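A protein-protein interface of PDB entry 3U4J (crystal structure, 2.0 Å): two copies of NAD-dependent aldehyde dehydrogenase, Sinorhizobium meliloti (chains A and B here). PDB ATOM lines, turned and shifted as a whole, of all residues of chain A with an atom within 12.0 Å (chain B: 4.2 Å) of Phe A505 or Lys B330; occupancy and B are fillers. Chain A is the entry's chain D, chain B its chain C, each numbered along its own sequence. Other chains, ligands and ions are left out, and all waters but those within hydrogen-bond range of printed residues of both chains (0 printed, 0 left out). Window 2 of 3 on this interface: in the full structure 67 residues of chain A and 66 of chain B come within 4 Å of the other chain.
The backbone NH (N) of Trp A504 sits at hydrogen-bond distance from the side-chain carboxylate (OD1) of Asp B290 (2.7 Å). The backbone NH of Phe A505 sits at hydrogen-bond distance from the side-chain carboxylate of Asp B290 (2.7 Å).
The backbone carbonyl oxygen of Val B331 is in hydrogen-bond range of the side-chain amide nitrogen of Asn B6, 2.8 Å away. OD1 of Asp B326 lies within salt-bridge range of NZ of Lys B330.
CA of Pro A503 touches OD1 of Asp B290 (3.3 Å). Val B331 touches Trp A504. CG2 of Ile B327 touches CG of Phe A505, 3.8 Å away. Lys B330 touches Phe A505.
Phe A505 touches just these residues of chain B: Asp B290, Ile B327 and Lys B330. Printed residues of chain A within 4 Å of Lys B330: Phe A505 (3.7 Å). Asn B6 touches none of the printed residues of chain A. Of chain A, only Pro A503 (3.3 Å), Trp A504 (2.7 Å) and Phe A505 (2.7 Å) come within 4 Å of Asp B290. Asp B326 touches none of the printed residues of chain A. No residue of chain A comes within 4 Å of Arg B329. No residue of chain A comes within 4 Å of Ala B332. Printed residues of chain B within 4 Å of Pro A503: Asp B290. Of the printed residues of chain B, Trp A504 touches Asp B290 and Val B331. Arg A500 touches none of the printed residues of chain B. Pro A501 touches none of the printed residues of chain B. The nearest printed residue of chain B that does not touch Phe A505 is Val B331 (4.2 Å). The nearest printed residue of chain B that does not touch Trp A504 is Ile B327 (5.1 Å).
Hydrophobic or aromatic side chains of chain A within 4 Å of the printed part of chain B: Pro A503, Trp A504 and Phe A505. Along chain A the printed residues that touch a printed residue of chain B span positions 503 to 505. Hydrophobic or aromatic side chains of chain B within 4 Å of the printed part of chain A: Ile B327 and Val B331. Along chain B the printed residues that touch a printed residue of chain A span positions 290 to 331. Among the printed residues, 6 pairs touch across the chains. Among the printed residues, no Asp or Glu carboxylate lies within 4 Å of a Lys or Arg side-chain nitrogen of the other chain.
No position is printed for both chains.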
ATOM      1  N   ARG A 500       7.747  14.661  33.215  1.00  0.00           N
ATOM      2  CA  ARG A 500       9.106  15.035  32.837  1.00  0.00           C
ATOM      3  C   ARG A 500       9.444  16.505  33.100  1.00  0.00           C
ATOM      4  O   ARG A 500       8.598  17.381  32.951  1.00  0.00           O
ATOM      5  CB  ARG A 500       9.390  14.648  31.366  1.00  0.00           C
ATOM      6  CG  ARG A 500       8.576  15.385  30.323  1.00  0.00           C
ATOM      7  CD  ARG A 500       8.362  14.515  29.061  1.00  0.00           C
ATOM      8  NE  ARG A 500       6.999  14.684  28.537  1.00  0.00           N
ATOM      9  CZ  ARG A 500       6.560  14.231  27.363  1.00  0.00           C
ATOM     10  NH1 ARG A 500       7.363  13.558  26.544  1.00  0.00           N
ATOM     11  NH2 ARG A 500       5.302  14.451  27.006  1.00  0.00           N
ATOM     12  N   PRO A 501      10.703  16.780  33.443  1.00  0.00           N
ATOM     13  CA  PRO A 501      11.101  18.178  33.534  1.00  0.00           C
ATOM     14  C   PRO A 501      11.226  18.824  32.148  1.00  0.00           C
ATOM     15  O   PRO A 501      11.218  18.110  31.126  1.00  0.00           O
ATOM     16  CB  PRO A 501      12.470  18.114  34.226  1.00  0.00           C
ATOM     17  CG  PRO A 501      12.955  16.702  34.055  1.00  0.00           C
ATOM     18  CD  PRO A 501      11.852  15.856  33.493  1.00  0.00           C
ATOM     19  N   ALA A 502      11.300  20.160  32.117  1.00  0.00           N
ATOM     20  CA  ALA A 502      11.691  20.901  30.907  1.00  0.00           C
ATOM     21  C   ALA A 502      13.121  20.497  30.548  1.00  0.00           C
ATOM     22  O   ALA A 502      13.964  20.376  31.445  1.00  0.00           O
ATOM     23  CB  ALA A 502      11.609  22.430  31.140  1.00  0.00           C
ATOM     24  N   PRO A 503      13.402  20.255  29.252  1.00  0.00           N
ATOM     25  CA  PRO A 503      14.742  19.766  28.918  1.00  0.00           C
ATOM     26  C   PRO A 503      15.804  20.854  29.053  1.00  0.00           C
ATOM     27  O   PRO A 503      15.519  22.019  28.817  1.00  0.00           O
ATOM     28  CB  PRO A 503      14.601  19.345  27.442  1.00  0.00           C
ATOM     29  CG  PRO A 503      13.547  20.258  26.900  1.00  0.00           C
ATOM     30  CD  PRO A 503      12.557  20.415  28.045  1.00  0.00           C
ATOM     31  N   TRP A 504      17.015  20.460  29.441  1.00  0.00           N
ATOM     32  CA  TRP A 504      18.168  21.362  29.472  1.00  0.00           C
ATOM     33  C   TRP A 504      18.698  21.627  28.061  1.00  0.00           C
ATOM     34  O   TRP A 504      18.967  22.777  27.671  1.00  0.00           O
ATOM     35  CB  TRP A 504      19.254  20.708  30.313  1.00  0.00           C
ATOM     36  CG  TRP A 504      20.544  21.438  30.459  1.00  0.00           C
ATOM     37  CD1 TRP A 504      20.764  22.633  31.107  1.00  0.00           C
ATOM     38  CD2 TRP A 504      21.829  20.976  30.021  1.00  0.00           C
ATOM     39  NE1 TRP A 504      22.116  22.939  31.081  1.00  0.00           N
ATOM     40  CE2 TRP A 504      22.786  21.935  30.428  1.00  0.00           C
ATOM     41  CE3 TRP A 504      22.259  19.844  29.315  1.00  0.00           C
ATOM     42  CZ2 TRP A 504      24.154  21.800  30.144  1.00  0.00           C
ATOM     43  CZ3 TRP A 504      23.628  19.699  29.043  1.00  0.00           C
ATOM     44  CH2 TRP A 504      24.555  20.679  29.459  1.00  0.00           C
ATOM     45  N   PHE A 505      18.866  20.559  27.293  1.00  0.00           N
ATOM     46  CA  PHE A 505      19.339  20.734  25.939  1.00  0.00           C
ATOM     47  C   PHE A 505      18.181  21.038  24.996  1.00  0.00           C
ATOM     48  O   PHE A 505      17.295  20.196  24.789  1.00  0.00           O
ATOM     49  CB  PHE A 505      20.137  19.526  25.456  1.00  0.00           C
ATOM     50  CG  PHE A 505      20.534  19.619  24.016  1.00  0.00           C
ATOM     51  CD1 PHE A 505      21.523  20.517  23.613  1.00  0.00           C
ATOM     52  CD2 PHE A 505      19.912  18.816  23.060  1.00  0.00           C
ATOM     53  CE1 PHE A 505      21.902  20.615  22.266  1.00  0.00           C
ATOM     54  CE2 PHE A 505      20.287  18.902  21.699  1.00  0.00           C
ATOM     55  CZ  PHE A 505      21.282  19.812  21.305  1.00  0.00           C
ATOM     56  N   THR A 506      18.206  22.250  24.452  1.00  0.00           N
ATOM     57  CA  THR A 506      17.300  22.675  23.390  1.00  0.00           C
ATOM     58  C   THR A 506      18.126  23.052  22.144  1.00  0.00           C
ATOM     59  O   THR A 506      17.576  23.252  21.056  1.00  0.00           O
ATOM     60  CB  THR A 506      16.424  23.887  23.821  1.00  0.00           C
ATOM     61  OG1 THR A 506      17.267  24.901  24.387  1.00  0.00           O
ATOM     62  CG2 THR A 506      15.372  23.475  24.862  1.00  0.00           C
ATOM     63  N   ASN B   6      31.211  21.583  18.085  1.00  0.00           N
ATOM     64  CA  ASN B   6      30.394  22.198  19.144  1.00  0.00           C
ATOM     65  C   ASN B   6      31.217  23.075  20.107  1.00  0.00           C
ATOM     66  O   ASN B   6      30.663  23.653  21.051  1.00  0.00           O
ATOM     67  CB  ASN B   6      29.554  21.157  19.898  1.00  0.00           C
ATOM     68  CG  ASN B   6      30.387  20.033  20.490  1.00  0.00           C
ATOM     69  OD1 ASN B   6      31.421  19.641  19.935  1.00  0.00           O
ATOM     70  ND2 ASN B   6      29.930  19.489  21.629  1.00  0.00           N
ATOM     71  N   ASP B 290      18.402  13.552  28.504  1.00  0.00           N
ATOM     72  CA  ASP B 290      18.638  14.983  28.727  1.00  0.00           C
ATOM     73  C   ASP B 290      19.103  15.231  30.153  1.00  0.00           C
ATOM     74  O   ASP B 290      20.086  15.963  30.377  1.00  0.00           O
ATOM     75  CB  ASP B 290      17.397  15.797  28.344  1.00  0.00           C
ATOM     76  CG  ASP B 290      17.566  17.301  28.603  1.00  0.00           C
ATOM     77  OD1 ASP B 290      17.274  17.747  29.740  1.00  0.00           O
ATOM     78  OD2 ASP B 290      17.990  18.029  27.670  1.00  0.00           O
ATOM     79  N   ASP B 326      24.128  11.577  21.314  1.00  0.00           N
ATOM     80  CA  ASP B 326      23.602  12.570  20.357  1.00  0.00           C
ATOM     81  C   ASP B 326      23.613  13.993  20.938  1.00  0.00           C
ATOM     82  O   ASP B 326      24.049  14.954  20.287  1.00  0.00           O
ATOM     83  CB  ASP B 326      22.196  12.157  19.882  1.00  0.00           C
ATOM     84  CG  ASP B 326      21.568  13.158  18.881  1.00  0.00           C
ATOM     85  OD1 ASP B 326      22.041  13.259  17.728  1.00  0.00           O
ATOM     86  OD2 ASP B 326      20.570  13.828  19.246  1.00  0.00           O
ATOM     87  N   ILE B 327      23.136  14.121  22.169  1.00  0.00           N
ATOM     88  CA  ILE B 327      23.145  15.402  22.854  1.00  0.00           C
ATOM     89  C   ILE B 327      24.593  15.844  23.081  1.00  0.00           C
ATOM     90  O   ILE B 327      24.927  16.995  22.830  1.00  0.00           O
ATOM     91  CB  ILE B 327      22.386  15.318  24.216  1.00  0.00           C
ATOM     92  CG1 ILE B 327      20.897  15.077  23.968  1.00  0.00           C
ATOM     93  CG2 ILE B 327      22.652  16.586  25.079  1.00  0.00           C
ATOM     94  CD1 ILE B 327      20.083  14.694  25.213  1.00  0.00           C
ATOM     95  N   SER B 328      25.442  14.930  23.547  1.00  0.00           N
ATOM     96  CA  SER B 328      26.815  15.282  23.902  1.00  0.00           C
ATOM     97  C   SER B 328      27.660  15.792  22.729  1.00  0.00           C
ATOM     98  O   SER B 328      28.599  16.592  22.927  1.00  0.00           O
ATOM     99  CB  SER B 328      27.521  14.097  24.569  1.00  0.00           C
ATOM    100  OG  SER B 328      26.835  13.647  25.725  1.00  0.00           O
ATOM    101  N   ARG B 329      27.317  15.340  21.520  1.00  0.00           N
ATOM    102  CA  ARG B 329      28.002  15.757  20.281  1.00  0.00           C
ATOM    103  C   ARG B 329      27.646  17.171  19.855  1.00  0.00           C
ATOM    104  O   ARG B 329      28.410  17.813  19.122  1.00  0.00           O
ATOM    105  CB  ARG B 329      27.592  14.831  19.112  1.00  0.00           C
ATOM    106  CG  ARG B 329      28.358  13.549  19.069  1.00  0.00           C
ATOM    107  CD  ARG B 329      28.186  12.852  17.720  1.00  0.00           C
ATOM    108  NE  ARG B 329      26.813  12.453  17.449  1.00  0.00           N
ATOM    109  CZ  ARG B 329      26.279  11.289  17.815  1.00  0.00           C
ATOM    110  NH1 ARG B 329      26.979  10.405  18.514  1.00  0.00           N
ATOM    111  NH2 ARG B 329      25.023  11.016  17.502  1.00  0.00           N
ATOM    112  N   LYS B 330      26.467  17.628  20.265  1.00  0.00           N
ATOM    113  CA  LYS B 330      25.902  18.878  19.767  1.00  0.00           C
ATOM    114  C   LYS B 330      26.033  19.996  20.812  1.00  0.00           C
ATOM    115  O   LYS B 330      26.102  21.162  20.460  1.00  0.00           O
ATOM    116  CB  LYS B 330      24.396  18.723  19.484  1.00  0.00           C
ATOM    117  CG  LYS B 330      23.926  17.796  18.349  1.00  0.00           C
ATOM    118  CD  LYS B 330      22.376  17.853  18.350  1.00  0.00           C
ATOM    119  CE  LYS B 330      21.709  17.406  17.038  1.00  0.00           C
ATOM    120  NZ  LYS B 330      21.415  15.937  16.987  1.00  0.00           N
ATOM    121  N   VAL B 331      26.022  19.636  22.096  1.00  0.00           N
ATOM    122  CA  VAL B 331      25.957  20.646  23.168  1.00  0.00           C
ATOM    123  C   VAL B 331      27.124  21.643  23.093  1.00  0.00           C
ATOM    124  O   VAL B 331      28.281  21.258  22.968  1.00  0.00           O
ATOM    125  CB  VAL B 331      25.796  20.002  24.583  1.00  0.00           C
ATOM    126  CG1 VAL B 331      27.008  19.164  24.948  1.00  0.00           C
ATOM    127  CG2 VAL B 331      25.532  21.077  25.661  1.00  0.00           C
ATOM    128  N   ALA B 332      26.792  22.931  23.132  1.00  0.00           N
ATOM    129  CA  ALA B 332      27.776  24.002  22.947  1.00  0.00           C
ATOM    130  C   ALA B 332      28.616  24.159  24.207  1.00  0.00           C
ATOM    131  O   ALA B 332      28.071  24.416  25.289  1.00  0.00           O
ATOM    132  CB  ALA B 332      27.067  25.314  22.616  1.00  0.00           C
